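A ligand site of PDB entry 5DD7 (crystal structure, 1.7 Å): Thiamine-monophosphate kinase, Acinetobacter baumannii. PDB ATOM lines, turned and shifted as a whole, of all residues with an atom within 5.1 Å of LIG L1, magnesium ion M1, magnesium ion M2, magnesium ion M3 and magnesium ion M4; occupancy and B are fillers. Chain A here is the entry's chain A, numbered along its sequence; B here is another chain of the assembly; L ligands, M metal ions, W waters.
O2 of LG2 L2 is bound to magnesium ion M4 (2.0 Å).
An oxygen (O3) of LIG L1 is bound to magnesium ion M4 (2.0 Å).
Magnesium ion M4 is bound by water W9, 2.1 Å away.
Magnesium ion M4 is bound by water W5 (2.1 Å).
OD1 of Asp 209 of chain B is bound to magnesium ion M4 (2.1 Å).
OD2 of Asp 209 of chain B binds magnesium ion M4, at 2.2 Å.
A nitrogen (N3) of LIG L1 sits at hydrogen-bond distance from the backbone NH (N) of Thr 127 (3.5 Å).
The side-chain hydroxyl of Thr 127 is in hydrogen-bond range of a nitrogen (N3) of LIG L1 (2.9 Å).
The side-chain hydroxyl (OG) of Ser 208 of chain B is in hydrogen-bond range of a nitrogen (N1) of LIG L1.
N of Asp 33 is in hydrogen-bond range of O11 of LIG L1, at 3.2 Å.
NH2 of Arg 151 of chain B sits close to O5 of LIG L1 (3.1 Å).
The backbone carbonyl oxygen (O) of Asp 33 lies within hydrogen-bond range of an oxygen (O11) of LIG L1 (2.6 Å).
The backbone NH (N) of Gly 125 lies within hydrogen-bond range of an oxygen (O12) of LIG L1, 3.0 Å away.
An oxygen (O12) of LIG L1 sits at hydrogen-bond distance from the backbone carbonyl oxygen (O) of Gly 125.
The backbone NH (N) of Gly 32 sits at hydrogen-bond distance from an oxygen (O11) of LIG L1 (2.9 Å).
N of Asp 126 lies within hydrogen-bond range of N3 of LIG L1 (3.2 Å).
An oxygen (O5) of LIG L1 is bound to magnesium ion M3 (2.0 Å).
The side-chain carboxylate (OD1) of Asp 206 of chain B binds magnesium ion M3, at 2.0 Å.
Magnesium ion M3 is bound by the side-chain carboxylate (OD1) of Asp 79 of chain B (2.0 Å).
Water W3 binds magnesium ion M3, at 2.1 Å.
The side-chain carboxylate (OD1) of Asp 34 is bound to magnesium ion M3 (2.1 Å).
Water W7 is bound to magnesium ion M3, at 2.1 Å.
Magnesium ion M3 has six donor atoms within binding distance.
One residue has an atom within 4 Å of magnesium ion M4: Asp 209 of chain B.
The backbone carbonyl oxygen of Asp 209 of chain B sits at hydrogen-bond distance from the backbone NH of Tyr 309 of chain B (2.8 Å).
NE of Arg 151 of chain B is in salt-bridge range of OD2 of Asp 34, at 3.1 Å.
The backbone NH (N) of Ile 94 lies within hydrogen-bond range of the backbone carbonyl oxygen (O) of Asp 126 (2.9 Å).
The backbone NH (N) of Ile 31 sits at hydrogen-bond distance from the backbone carbonyl oxygen (O) of Ile 123 (3.4 Å).
The backbone carbonyl oxygen (O) of Leu 92 is in hydrogen-bond range of the backbone NH (N) of Asp 126, at 2.9 Å.
OD1 of Asp 33 lies within salt-bridge range of NE of Arg 151 of chain B.
The backbone NH (N) of Leu 92 lies within hydrogen-bond range of the backbone carbonyl oxygen (O) of Gly 124 (2.9 Å).
Magnesium ion M2 is bound by O2 of LIG L1 (2.0 Å), OD2 of Asp 51 of chain B (2.0 Å), OD2 of Asp 79 of chain B (2.1 Å), water W10 (2.1 Å), O4 of LIG L1 (2.2 Å) and water W7 (2.3 Å).
Within 4 Å of magnesium ion M2: Asp 51 of chain B and Asp 79 of chain B.
Magnesium ion M1 is bound by OD1 of Asp 51 of chain B (2.0 Å), OD1 of Asp 126 (2.1 Å), O7 of LIG L1 (2.1 Å), O1 of LIG L1 (2.1 Å), water W8 (2.2 Å) and O4 of LIG L1 (2.5 Å).
Magnesium ion M1 has six donor atoms within binding distance.
Water W8 lies within hydrogen-bond range of O of Gly 125 (2.6 Å) and O of Ala 50 of chain B (2.8 Å).
Water W7 lies within hydrogen-bond range of OD2 of Asp 206 of chain B (2.7 Å), OG of Ser 208 of chain B (3.1 Å) and N1 of LIG L1 (3.2 Å).
Water W3 lies within hydrogen-bond range of the backbone carbonyl oxygen of Asp 206 of chain B (2.8 Å), the side-chain hydroxyl of Ser 208 of chain B (3.3 Å) and the guanidinium group of Arg 151 of chain B (3.5 Å).
Water W5 bridges the side-chain carboxylate of Glu 11 (2.8 Å) and the backbone carbonyl oxygen of Tyr 309 of chain B (3.0 Å).
Water W11 lies within hydrogen-bond range of O of Gly 30 (2.6 Å), N of Asp 33 (2.9 Å), O11 of LIG L1 (3.3 Å) and N of Gly 32 (3.4 Å).
Water W1 lies within hydrogen-bond range of the backbone NH of Ala 50 of chain B (3.0 Å), the backbone carbonyl oxygen of Gly 125 (3.1 Å) and an oxygen (O12) of LIG L1 (3.4 Å).
Of the 29 residues printed, 2 come within 4 Å of magnesium ion M1.
Arg 151 of chain B touches magnesium ion M3 (NH2 to MG, 3.7 Å).
The nearest printed residue that does not touch magnesium ion M3 is Ser 208 of chain B (4.4 Å).
O of Gly 124 lies close to N6 of LIG L1, 3.5 Å away.
Merely in contact with LIG L1: Glu 11 (3.9 Å), Phe 12 (3.5 Å), Ile 15 (3.4 Å), Phe 19 (3.4 Å), Ile 31 (3.5 Å), Leu 92 (3.5 Å) and Ile 94 (3.8 Å).
Hydrophobic or aromatic side chains that line LIG L1: Phe 12, Ile 15, Phe 19, Ile 31, Leu 92 and Ile 94.
Of the 29 residues printed, 20 come within 4 Å of LIG L1.
The nearest printed residue that does not touch LIG L1 is Leu 122 (4.1 Å).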
ATOM      1  N   GLU A  11     -20.440  26.466 -15.152  1.00  0.00           N
ATOM      2  CA  GLU A  11     -19.934  25.338 -15.944  1.00  0.00           C
ATOM      3  C   GLU A  11     -18.881  24.520 -15.193  1.00  0.00           C
ATOM      4  O   GLU A  11     -18.973  23.294 -15.105  1.00  0.00           O
ATOM      5  CB  GLU A  11     -19.369  25.892 -17.254  1.00  0.00           C
ATOM      6  CG  GLU A  11     -18.734  24.861 -18.163  1.00  0.00           C
ATOM      7  CD  GLU A  11     -17.986  25.517 -19.310  1.00  0.00           C
ATOM      8  OE1 GLU A  11     -18.156  26.749 -19.507  1.00  0.00           O
ATOM      9  OE2 GLU A  11     -17.231  24.819 -20.002  1.00  0.00           O
ATOM     10  N   PHE A  12     -17.838  25.172 -14.683  1.00  0.00           N
ATOM     11  CA  PHE A  12     -16.724  24.401 -14.147  1.00  0.00           C
ATOM     12  C   PHE A  12     -17.079  23.744 -12.820  1.00  0.00           C
ATOM     13  O   PHE A  12     -16.635  22.624 -12.542  1.00  0.00           O
ATOM     14  CB  PHE A  12     -15.493  25.318 -14.024  1.00  0.00           C
ATOM     15  CG  PHE A  12     -15.032  25.851 -15.357  1.00  0.00           C
ATOM     16  CD1 PHE A  12     -14.858  25.000 -16.434  1.00  0.00           C
ATOM     17  CD2 PHE A  12     -14.810  27.208 -15.532  1.00  0.00           C
ATOM     18  CE1 PHE A  12     -14.440  25.485 -17.665  1.00  0.00           C
ATOM     19  CE2 PHE A  12     -14.394  27.706 -16.758  1.00  0.00           C
ATOM     20  CZ  PHE A  12     -14.223  26.850 -17.826  1.00  0.00           C
ATOM     21  N   ILE A  15     -19.069  20.552 -13.647  1.00  0.00           N
ATOM     22  CA  ILE A  15     -18.180  19.438 -13.983  1.00  0.00           C
ATOM     23  C   ILE A  15     -17.592  18.831 -12.723  1.00  0.00           C
ATOM     24  O   ILE A  15     -17.605  17.604 -12.539  1.00  0.00           O
ATOM     25  CB  ILE A  15     -17.080  19.899 -14.949  1.00  0.00           C
ATOM     26  CG1 ILE A  15     -17.672  20.437 -16.270  1.00  0.00           C
ATOM     27  CG2 ILE A  15     -16.071  18.772 -15.180  1.00  0.00           C
ATOM     28  CD1 ILE A  15     -16.691  21.236 -17.110  1.00  0.00           C
ATOM     29  N   PHE A  19     -19.525  15.390 -12.518  1.00  0.00           N
ATOM     30  CA  PHE A  19     -18.962  14.596 -13.598  1.00  0.00           C
ATOM     31  C   PHE A  19     -17.474  14.323 -13.416  1.00  0.00           C
ATOM     32  O   PHE A  19     -16.771  14.080 -14.404  1.00  0.00           O
ATOM     33  CB  PHE A  19     -19.211  15.280 -14.950  1.00  0.00           C
ATOM     34  CG  PHE A  19     -20.664  15.523 -15.243  1.00  0.00           C
ATOM     35  CD1 PHE A  19     -21.554  14.459 -15.328  1.00  0.00           C
ATOM     36  CD2 PHE A  19     -21.157  16.804 -15.393  1.00  0.00           C
ATOM     37  CE1 PHE A  19     -22.887  14.678 -15.593  1.00  0.00           C
ATOM     38  CE2 PHE A  19     -22.504  17.037 -15.644  1.00  0.00           C
ATOM     39  CZ  PHE A  19     -23.371  15.970 -15.747  1.00  0.00           C
ATOM     40  N   GLY A  30      -7.339  11.469 -17.030  1.00  0.00           N
ATOM     41  CA  GLY A  30      -8.757  11.710 -17.089  1.00  0.00           C
ATOM     42  C   GLY A  30      -9.070  13.188 -17.062  1.00  0.00           C
ATOM     43  O   GLY A  30      -8.261  14.026 -17.478  1.00  0.00           O
ATOM     44  N   ILE A  31     -10.230  13.515 -16.502  1.00  0.00           N
ATOM     45  CA  ILE A  31     -10.780  14.865 -16.588  1.00  0.00           C
ATOM     46  C   ILE A  31      -9.836  15.897 -15.970  1.00  0.00           C
ATOM     47  O   ILE A  31      -9.263  15.689 -14.895  1.00  0.00           O
ATOM     48  CB  ILE A  31     -12.149  14.867 -15.905  1.00  0.00           C
ATOM     49  CG1 ILE A  31     -13.146  14.083 -16.765  1.00  0.00           C
ATOM     50  CG2 ILE A  31     -12.630  16.288 -15.659  1.00  0.00           C
ATOM     51  CD1 ILE A  31     -14.328  13.590 -15.962  1.00  0.00           C
ATOM     52  N   GLY A  32      -9.701  17.039 -16.655  1.00  0.00           N
ATOM     53  CA  GLY A  32      -8.974  18.170 -16.118  1.00  0.00           C
ATOM     54  C   GLY A  32      -8.029  18.827 -17.103  1.00  0.00           C
ATOM     55  O   GLY A  32      -7.449  19.879 -16.811  1.00  0.00           O
ATOM     56  N   ASP A  33      -7.854  18.237 -18.265  1.00  0.00           N
ATOM     57  CA  ASP A  33      -6.963  18.806 -19.256  1.00  0.00           C
ATOM     58  C   ASP A  33      -7.718  18.989 -20.573  1.00  0.00           C
ATOM     59  O   ASP A  33      -8.904  18.670 -20.683  1.00  0.00           O
ATOM     60  CB  ASP A  33      -5.722  17.921 -19.435  1.00  0.00           C
ATOM     61  CG  ASP A  33      -4.452  18.726 -19.606  1.00  0.00           C
ATOM     62  OD1 ASP A  33      -4.346  19.429 -20.615  1.00  0.00           O
ATOM     63  OD2 ASP A  33      -3.569  18.679 -18.717  1.00  0.00           O
ATOM     64  N   ASP A  34      -7.002  19.473 -21.586  1.00  0.00           N
ATOM     65  CA  ASP A  34      -7.672  19.750 -22.859  1.00  0.00           C
ATOM     66  C   ASP A  34      -8.171  18.484 -23.545  1.00  0.00           C
ATOM     67  O   ASP A  34      -9.233  18.521 -24.168  1.00  0.00           O
ATOM     68  CB  ASP A  34      -6.714  20.522 -23.756  1.00  0.00           C
ATOM     69  CG  ASP A  34      -6.358  21.853 -23.144  1.00  0.00           C
ATOM     70  OD1 ASP A  34      -7.160  22.800 -23.304  1.00  0.00           O
ATOM     71  OD2 ASP A  34      -5.304  21.969 -22.477  1.00  0.00           O
ATOM     72  N   LEU A  92     -18.524  12.640 -22.386  1.00  0.00           N
ATOM     73  CA  LEU A  92     -19.895  13.114 -22.221  1.00  0.00           C
ATOM     74  C   LEU A  92     -19.996  14.576 -22.663  1.00  0.00           C
ATOM     75  O   LEU A  92     -19.448  15.457 -22.011  1.00  0.00           O
ATOM     76  CB  LEU A  92     -20.319  12.993 -20.764  1.00  0.00           C
ATOM     77  CG  LEU A  92     -21.599  13.709 -20.370  1.00  0.00           C
ATOM     78  CD1 LEU A  92     -22.793  13.087 -21.092  1.00  0.00           C
ATOM     79  CD2 LEU A  92     -21.798  13.619 -18.855  1.00  0.00           C
ATOM     80  N   ILE A  94     -22.690  17.472 -23.024  1.00  0.00           N
ATOM     81  CA  ILE A  94     -24.061  17.762 -22.626  1.00  0.00           C
ATOM     82  C   ILE A  94     -24.339  19.252 -22.817  1.00  0.00           C
ATOM     83  O   ILE A  94     -23.528  20.105 -22.446  1.00  0.00           O
ATOM     84  CB  ILE A  94     -24.359  17.323 -21.176  1.00  0.00           C
ATOM     85  CG1 ILE A  94     -25.783  17.727 -20.795  1.00  0.00           C
ATOM     86  CG2 ILE A  94     -23.343  17.890 -20.213  1.00  0.00           C
ATOM     87  CD1 ILE A  94     -26.408  16.825 -19.760  1.00  0.00           C
ATOM     88  N   LEU A 122     -15.585   7.489 -17.124  1.00  0.00           N
ATOM     89  CA  LEU A 122     -15.911   8.761 -17.766  1.00  0.00           C
ATOM     90  C   LEU A 122     -14.670   9.627 -17.702  1.00  0.00           C
ATOM     91  O   LEU A 122     -14.234  10.023 -16.612  1.00  0.00           O
ATOM     92  CB  LEU A 122     -17.091   9.438 -17.063  1.00  0.00           C
ATOM     93  CG  LEU A 122     -17.392  10.879 -17.489  1.00  0.00           C
ATOM     94  CD1 LEU A 122     -17.710  10.958 -18.973  1.00  0.00           C
ATOM     95  CD2 LEU A 122     -18.565  11.424 -16.665  1.00  0.00           C
ATOM     96  N   ILE A 123     -14.044   9.881 -18.844  1.00  0.00           N
ATOM     97  CA  ILE A 123     -12.703  10.450 -18.844  1.00  0.00           C
ATOM     98  C   ILE A 123     -12.650  11.845 -19.446  1.00  0.00           C
ATOM     99  O   ILE A 123     -11.567  12.437 -19.486  1.00  0.00           O
ATOM    100  CB  ILE A 123     -11.688   9.533 -19.552  1.00  0.00           C
ATOM    101  CG1 ILE A 123     -11.984   9.440 -21.048  1.00  0.00           C
ATOM    102  CG2 ILE A 123     -11.747   8.129 -18.933  1.00  0.00           C
ATOM    103  CD1 ILE A 123     -10.933   8.625 -21.808  1.00  0.00           C
ATOM    104  N   GLY A 124     -13.771  12.382 -19.908  1.00  0.00           N
ATOM    105  CA  GLY A 124     -13.750  13.714 -20.495  1.00  0.00           C
ATOM    106  C   GLY A 124     -15.117  14.060 -21.058  1.00  0.00           C
ATOM    107  O   GLY A 124     -16.080  13.288 -20.967  1.00  0.00           O
ATOM    108  N   GLY A 125     -15.176  15.236 -21.672  1.00  0.00           N
ATOM    109  CA  GLY A 125     -16.415  15.673 -22.286  1.00  0.00           C
ATOM    110  C   GLY A 125     -16.432  17.179 -22.452  1.00  0.00           C
ATOM    111  O   GLY A 125     -15.377  17.819 -22.523  1.00  0.00           O
ATOM    112  N   ASP A 126     -17.647  17.713 -22.534  1.00  0.00           N
ATOM    113  CA  ASP A 126     -17.868  19.130 -22.745  1.00  0.00           C
ATOM    114  C   ASP A 126     -19.221  19.499 -22.181  1.00  0.00           C
ATOM    115  O   ASP A 126     -20.180  18.730 -22.287  1.00  0.00           O
ATOM    116  CB  ASP A 126     -17.790  19.492 -24.239  1.00  0.00           C
ATOM    117  CG  ASP A 126     -17.714  20.992 -24.471  1.00  0.00           C
ATOM    118  OD1 ASP A 126     -16.905  21.705 -23.807  1.00  0.00           O
ATOM    119  OD2 ASP A 126     -18.485  21.475 -25.339  1.00  0.00           O
ATOM    120  N   THR A 127     -19.293  20.672 -21.573  1.00  0.00           N
ATOM    121  CA  THR A 127     -20.514  21.183 -20.960  1.00  0.00           C
ATOM    122  C   THR A 127     -20.835  22.543 -21.566  1.00  0.00           C
ATOM    123  O   THR A 127     -19.980  23.432 -21.585  1.00  0.00           O
ATOM    124  CB  THR A 127     -20.322  21.319 -19.453  1.00  0.00           C
ATOM    125  OG1 THR A 127     -19.884  20.057 -18.934  1.00  0.00           O
ATOM    126  CG2 THR A 127     -21.635  21.752 -18.783  1.00  0.00           C
ATOM    127  N   ALA B  50     -13.720  16.165 -26.971  1.00  0.00           N
ATOM    128  CA  ALA B  50     -14.957  16.462 -27.693  1.00  0.00           C
ATOM    129  C   ALA B  50     -15.466  17.831 -27.259  1.00  0.00           C
ATOM    130  O   ALA B  50     -15.360  18.178 -26.084  1.00  0.00           O
ATOM    131  CB  ALA B  50     -16.012  15.404 -27.453  1.00  0.00           C
ATOM    132  N   ASP B  51     -15.981  18.601 -28.231  1.00  0.00           N
ATOM    133  CA  ASP B  51     -16.480  19.946 -27.984  1.00  0.00           C
ATOM    134  C   ASP B  51     -17.744  20.162 -28.806  1.00  0.00           C
ATOM    135  O   ASP B  51     -17.796  19.787 -29.979  1.00  0.00           O
ATOM    136  CB  ASP B  51     -15.457  21.036 -28.348  1.00  0.00           C
ATOM    137  CG  ASP B  51     -14.671  21.544 -27.139  1.00  0.00           C
ATOM    138  OD1 ASP B  51     -15.242  21.618 -26.030  1.00  0.00           O
ATOM    139  OD2 ASP B  51     -13.491  21.923 -27.307  1.00  0.00           O
ATOM    140  N   VAL B  75     -12.016  23.689 -33.584  1.00  0.00           N
ATOM    141  CA  VAL B  75     -11.927  23.875 -32.133  1.00  0.00           C
ATOM    142  C   VAL B  75     -11.514  22.584 -31.460  1.00  0.00           C
ATOM    143  O   VAL B  75     -10.900  22.615 -30.385  1.00  0.00           O
ATOM    144  CB  VAL B  75     -13.231  24.443 -31.530  1.00  0.00           C
ATOM    145  CG1 VAL B  75     -13.638  25.745 -32.243  1.00  0.00           C
ATOM    146  CG2 VAL B  75     -14.365  23.416 -31.572  1.00  0.00           C
ATOM    147  N   ASP B  79      -7.745  21.313 -29.226  1.00  0.00           N
ATOM    148  CA  ASP B  79      -7.547  20.616 -27.957  1.00  0.00           C
ATOM    149  C   ASP B  79      -6.578  19.445 -28.094  1.00  0.00           C
ATOM    150  O   ASP B  79      -5.903  19.093 -27.107  1.00  0.00           O
ATOM    151  CB  ASP B  79      -8.883  20.148 -27.393  1.00  0.00           C
ATOM    152  CG  ASP B  79      -9.554  21.220 -26.557  1.00  0.00           C
ATOM    153  OD1 ASP B  79      -8.852  21.861 -25.756  1.00  0.00           O
ATOM    154  OD2 ASP B  79     -10.775  21.414 -26.715  1.00  0.00           O
ATOM    155  N   ALA B  82      -3.263  21.299 -28.033  1.00  0.00           N
ATOM    156  CA  ALA B  82      -2.978  21.777 -26.692  1.00  0.00           C
ATOM    157  C   ALA B  82      -2.289  20.728 -25.820  1.00  0.00           C
ATOM    158  O   ALA B  82      -1.771  21.067 -24.757  1.00  0.00           O
ATOM    159  CB  ALA B  82      -4.274  22.232 -26.028  1.00  0.00           C
ATOM    160  N   ARG B 151      -1.695  20.754 -18.366  1.00  0.00           N
ATOM    161  CA  ARG B 151      -1.920  22.057 -17.752  1.00  0.00           C
ATOM    162  C   ARG B 151      -1.176  22.214 -16.437  1.00  0.00           C
ATOM    163  O   ARG B 151      -1.031  23.337 -15.959  1.00  0.00           O
ATOM    164  CB  ARG B 151      -3.401  22.309 -17.519  1.00  0.00           C
ATOM    165  CG  ARG B 151      -4.232  22.353 -18.793  1.00  0.00           C
ATOM    166  CD  ARG B 151      -5.695  22.554 -18.438  1.00  0.00           C
ATOM    167  NE  ARG B 151      -6.524  22.578 -19.651  1.00  0.00           N
ATOM    168  CZ  ARG B 151      -7.808  22.896 -19.658  1.00  0.00           C
ATOM    169  NH1 ARG B 151      -8.421  23.215 -18.516  1.00  0.00           N
ATOM    170  NH2 ARG B 151      -8.478  22.912 -20.810  1.00  0.00           N
ATOM    171  N   ILE B 205      -2.268  25.240 -22.741  1.00  0.00           N
ATOM    172  CA  ILE B 205      -3.718  25.207 -22.895  1.00  0.00           C
ATOM    173  C   ILE B 205      -4.039  25.974 -24.169  1.00  0.00           C
ATOM    174  O   ILE B 205      -3.285  26.855 -24.569  1.00  0.00           O
ATOM    175  CB  ILE B 205      -4.416  25.827 -21.670  1.00  0.00           C
ATOM    176  CG1 ILE B 205      -5.934  25.593 -21.694  1.00  0.00           C
ATOM    177  CG2 ILE B 205      -4.139  27.342 -21.590  1.00  0.00           C
ATOM    178  CD1 ILE B 205      -6.615  25.925 -20.368  1.00  0.00           C
ATOM    179  N   ASP B 206      -5.154  25.641 -24.841  1.00  0.00           N
ATOM    180  CA  ASP B 206      -5.572  26.483 -25.943  1.00  0.00           C
ATOM    181  C   ASP B 206      -6.585  27.521 -25.465  1.00  0.00           C
ATOM    182  O   ASP B 206      -7.363  27.279 -24.545  1.00  0.00           O
ATOM    183  CB  ASP B 206      -6.167  25.677 -27.114  1.00  0.00           C
ATOM    184  CG  ASP B 206      -7.399  24.907 -26.723  1.00  0.00           C
ATOM    185  OD1 ASP B 206      -7.412  24.373 -25.604  1.00  0.00           O
ATOM    186  OD2 ASP B 206      -8.353  24.851 -27.524  1.00  0.00           O
ATOM    187  N   SER B 208      -9.557  29.139 -25.675  1.00  0.00           N
ATOM    188  CA  SER B 208     -10.924  29.091 -26.175  1.00  0.00           C
ATOM    189  C   SER B 208     -11.857  30.033 -25.426  1.00  0.00           C
ATOM    190  O   SER B 208     -12.806  30.559 -26.024  1.00  0.00           O
ATOM    191  CB  SER B 208     -11.476  27.664 -26.078  1.00  0.00           C
ATOM    192  OG  SER B 208     -11.252  27.118 -24.780  1.00  0.00           O
ATOM    193  N   ASP B 209     -11.605  30.285 -24.144  1.00  0.00           N
ATOM    194  CA  ASP B 209     -12.491  31.081 -23.315  1.00  0.00           C
ATOM    195  C   ASP B 209     -11.955  32.475 -22.998  1.00  0.00           C
ATOM    196  O   ASP B 209     -12.748  33.346 -22.617  1.00  0.00           O
ATOM    197  CB  ASP B 209     -12.795  30.358 -21.993  1.00  0.00           C
ATOM    198  CG  ASP B 209     -13.560  29.068 -22.215  1.00  0.00           C
ATOM    199  OD1 ASP B 209     -14.402  29.038 -23.142  1.00  0.00           O
ATOM    200  OD2 ASP B 209     -13.315  28.100 -21.463  1.00  0.00           O
ATOM    201  N   TYR B 258      -8.331  30.383 -30.069  1.00  0.00           N
ATOM    202  CA  TYR B 258      -7.781  29.082 -30.441  1.00  0.00           C
ATOM    203  C   TYR B 258      -6.282  29.197 -30.759  1.00  0.00           C
ATOM    204  O   TYR B 258      -5.745  28.502 -31.617  1.00  0.00           O
ATOM    205  CB  TYR B 258      -8.612  28.424 -31.567  1.00  0.00           C
ATOM    206  CG  TYR B 258      -9.999  28.191 -31.003  1.00  0.00           C
ATOM    207  CD1 TYR B 258     -10.220  27.155 -30.102  1.00  0.00           C
ATOM    208  CD2 TYR B 258     -11.047  29.067 -31.284  1.00  0.00           C
ATOM    209  CE1 TYR B 258     -11.473  26.951 -29.537  1.00  0.00           C
ATOM    210  CE2 TYR B 258     -12.287  28.896 -30.697  1.00  0.00           C
ATOM    211  CZ  TYR B 258     -12.494  27.831 -29.831  1.00  0.00           C
ATOM    212  OH  TYR B 258     -13.726  27.638 -29.263  1.00  0.00           O
ATOM    213  N   TYR B 309     -14.938  33.455 -20.809  1.00  0.00           N
ATOM    214  CA  TYR B 309     -16.224  32.847 -21.118  1.00  0.00           C
ATOM    215  C   TYR B 309     -16.465  31.618 -20.255  1.00  0.00           C
ATOM    216  O   TYR B 309     -15.608  30.732 -20.150  1.00  0.00           O
ATOM    217  CB  TYR B 309     -16.298  32.481 -22.600  1.00  0.00           C
ATOM    218  CG  TYR B 309     -17.704  32.160 -23.057  1.00  0.00           C
ATOM    219  CD1 TYR B 309     -18.250  30.901 -22.857  1.00  0.00           C
ATOM    220  CD2 TYR B 309     -18.487  33.132 -23.682  1.00  0.00           C
ATOM    221  CE1 TYR B 309     -19.534  30.606 -23.260  1.00  0.00           C
ATOM    222  CE2 TYR B 309     -19.773  32.834 -24.098  1.00  0.00           C
ATOM    223  CZ  TYR B 309     -20.284  31.571 -23.889  1.00  0.00           C
ATOM    224  OH  TYR B 309     -21.574  31.270 -24.296  1.00  0.00           O
HETATM  225  P1  LIG L   1     -13.515  24.751 -24.153  1.00  0.00           P
HETATM  226  O1  LIG L   1     -14.728  23.968 -23.916  1.00  0.00           O
HETATM  227  O2  LIG L   1     -13.104  24.569 -25.610  1.00  0.00           O
HETATM  228  O3  LIG L   1     -13.779  26.271 -23.793  1.00  0.00           O
HETATM  229  P2  LIG L   1     -11.657  22.699 -23.168  1.00  0.00           P
HETATM  230  O4  LIG L   1     -12.380  22.005 -24.336  1.00  0.00           O
HETATM  231  O5  LIG L   1     -10.210  22.682 -23.325  1.00  0.00           O
HETATM  232  N1  LIG L   1     -12.286  24.207 -23.186  1.00  0.00           N
HETATM  233  P3  LIG L   1     -13.506  22.118 -21.032  1.00  0.00           P
HETATM  234  O6  LIG L   1     -13.567  23.435 -20.332  1.00  0.00           O
HETATM  235  O7  LIG L   1     -14.670  21.873 -21.993  1.00  0.00           O
HETATM  236  O8  LIG L   1     -12.137  21.990 -21.840  1.00  0.00           O
HETATM  237  O9  LIG L   1     -13.516  20.952 -19.987  1.00  0.00           O
HETATM  238  C1  LIG L   1     -12.640  20.964 -18.845  1.00  0.00           C
HETATM  239  C2  LIG L   1     -12.350  19.529 -18.491  1.00  0.00           C
HETATM  240  O10 LIG L   1     -13.568  18.894 -18.058  1.00  0.00           O
HETATM  241  C3  LIG L   1     -11.832  18.695 -19.666  1.00  0.00           C
HETATM  242  O11 LIG L   1     -10.881  17.713 -19.249  1.00  0.00           O
HETATM  243  C4  LIG L   1     -13.117  18.055 -20.216  1.00  0.00           C
HETATM  244  O12 LIG L   1     -12.819  16.837 -20.877  1.00  0.00           O
HETATM  245  C5  LIG L   1     -13.912  17.831 -18.926  1.00  0.00           C
HETATM  246  N2  LIG L   1     -15.368  17.844 -19.094  1.00  0.00           N
HETATM  247  C6  LIG L   1     -16.141  18.913 -19.475  1.00  0.00           C
HETATM  248  N3  LIG L   1     -17.430  18.682 -19.444  1.00  0.00           N
HETATM  249  C7  LIG L   1     -17.516  17.372 -19.009  1.00  0.00           C
HETATM  250  C8  LIG L   1     -18.615  16.538 -18.724  1.00  0.00           C
HETATM  251  N4  LIG L   1     -19.893  16.906 -18.856  1.00  0.00           N
HETATM  252  N5  LIG L   1     -18.346  15.287 -18.279  1.00  0.00           N
HETATM  253  C9  LIG L   1     -17.077  14.907 -18.144  1.00  0.00           C
HETATM  254  N6  LIG L   1     -15.965  15.603 -18.380  1.00  0.00           N
HETATM  255  C10 LIG L   1     -16.256  16.840 -18.804  1.00  0.00           C
HETATM  256  C1  LG2 L   2     -23.040  34.300 -31.162  1.00  0.00           C
HETATM  257  N1  LG2 L   2     -18.201  32.370 -27.472  1.00  0.00           N
HETATM  258  C2  LG2 L   2     -19.147  31.449 -27.549  1.00  0.00           C
HETATM  259  S1  LG2 L   2     -18.712  30.028 -26.771  1.00  0.00           S
HETATM  260  C3  LG2 L   2     -17.165  30.693 -26.320  1.00  0.00           C
HETATM  261  C4  LG2 L   2     -17.073  31.961 -26.764  1.00  0.00           C
HETATM  262  C5  LG2 L   2     -15.915  32.892 -26.587  1.00  0.00           C
HETATM  263  C6  LG2 L   2     -16.134  29.912 -25.557  1.00  0.00           C
HETATM  264  C7  LG2 L   2     -15.913  28.536 -26.152  1.00  0.00           C
HETATM  265  O1  LG2 L   2     -17.107  27.762 -25.926  1.00  0.00           O
HETATM  266  N2  LG2 L   2     -21.887  34.600 -29.053  1.00  0.00           N
HETATM  267  C8  LG2 L   2     -21.811  34.169 -30.319  1.00  0.00           C
HETATM  268  N3  LG2 L   2     -20.736  33.628 -30.902  1.00  0.00           N
HETATM  269  C9  LG2 L   2     -19.619  33.503 -30.164  1.00  0.00           C
HETATM  270  N4  LG2 L   2     -18.565  32.951 -30.749  1.00  0.00           N
HETATM  271  C10 LG2 L   2     -19.593  33.932 -28.807  1.00  0.00           C
HETATM  272  C11 LG2 L   2     -20.765  34.468 -28.330  1.00  0.00           C
HETATM  273  C12 LG2 L   2     -18.362  33.754 -27.964  1.00  0.00           C
HETATM  274  P1  LG2 L   2     -17.113  26.429 -25.051  1.00  0.00           P
HETATM  275  O2  LG2 L   2     -16.523  26.728 -23.689  1.00  0.00           O
HETATM  276  O3  LG2 L   2     -18.542  25.938 -24.969  1.00  0.00           O
HETATM  277  O4  LG2 L   2     -16.230  25.406 -25.836  1.00  0.00           O
HETATM  278 MG    MG M   1     -14.865  21.906 -24.049  1.00  0.00          MG
HETATM  279 MG    MG M   2     -12.048  22.983 -26.328  1.00  0.00          MG
HETATM  280 MG    MG M   3      -8.807  23.432 -24.461  1.00  0.00          MG
HETATM  281 MG    MG M   4     -15.008  27.095 -22.510  1.00  0.00          MG
HETATM  282  O   HOH W   1     -12.976  17.013 -24.227  1.00  0.00           O
HETATM  283  O   HOH W   2     -11.438  14.813 -23.228  1.00  0.00           O
HETATM  284  O   HOH W   3      -8.896  25.204 -23.364  1.00  0.00           O
HETATM  285  O   HOH W   4     -11.055  24.296 -19.663  1.00  0.00           O
HETATM  286  O   HOH W   5     -16.301  28.027 -21.132  1.00  0.00           O
HETATM  287  O   HOH W   6     -17.005  22.116 -20.589  1.00  0.00           O
HETATM  288  O   HOH W   7     -10.296  24.287 -25.753  1.00  0.00           O
HETATM  289  O   HOH W   8     -14.462  19.753 -24.013  1.00  0.00           O
HETATM  290  O   HOH W   9     -15.081  25.444 -21.282  1.00  0.00           O
HETATM  291  O   HOH W  10     -11.735  23.939 -28.161  1.00  0.00           O
HETATM  292  O   HOH W  11      -8.320  15.655 -19.494  1.00  0.00           O
HETATM  293  O   HOH W  12     -14.206  25.305 -28.075  1.00  0.00           O
HETATM  294  O   HOH W  13     -10.769  14.934 -20.457  1.00  0.00           O
HETATM  295  O   HOH W  14     -10.877  26.440 -21.598  1.00  0.00           O
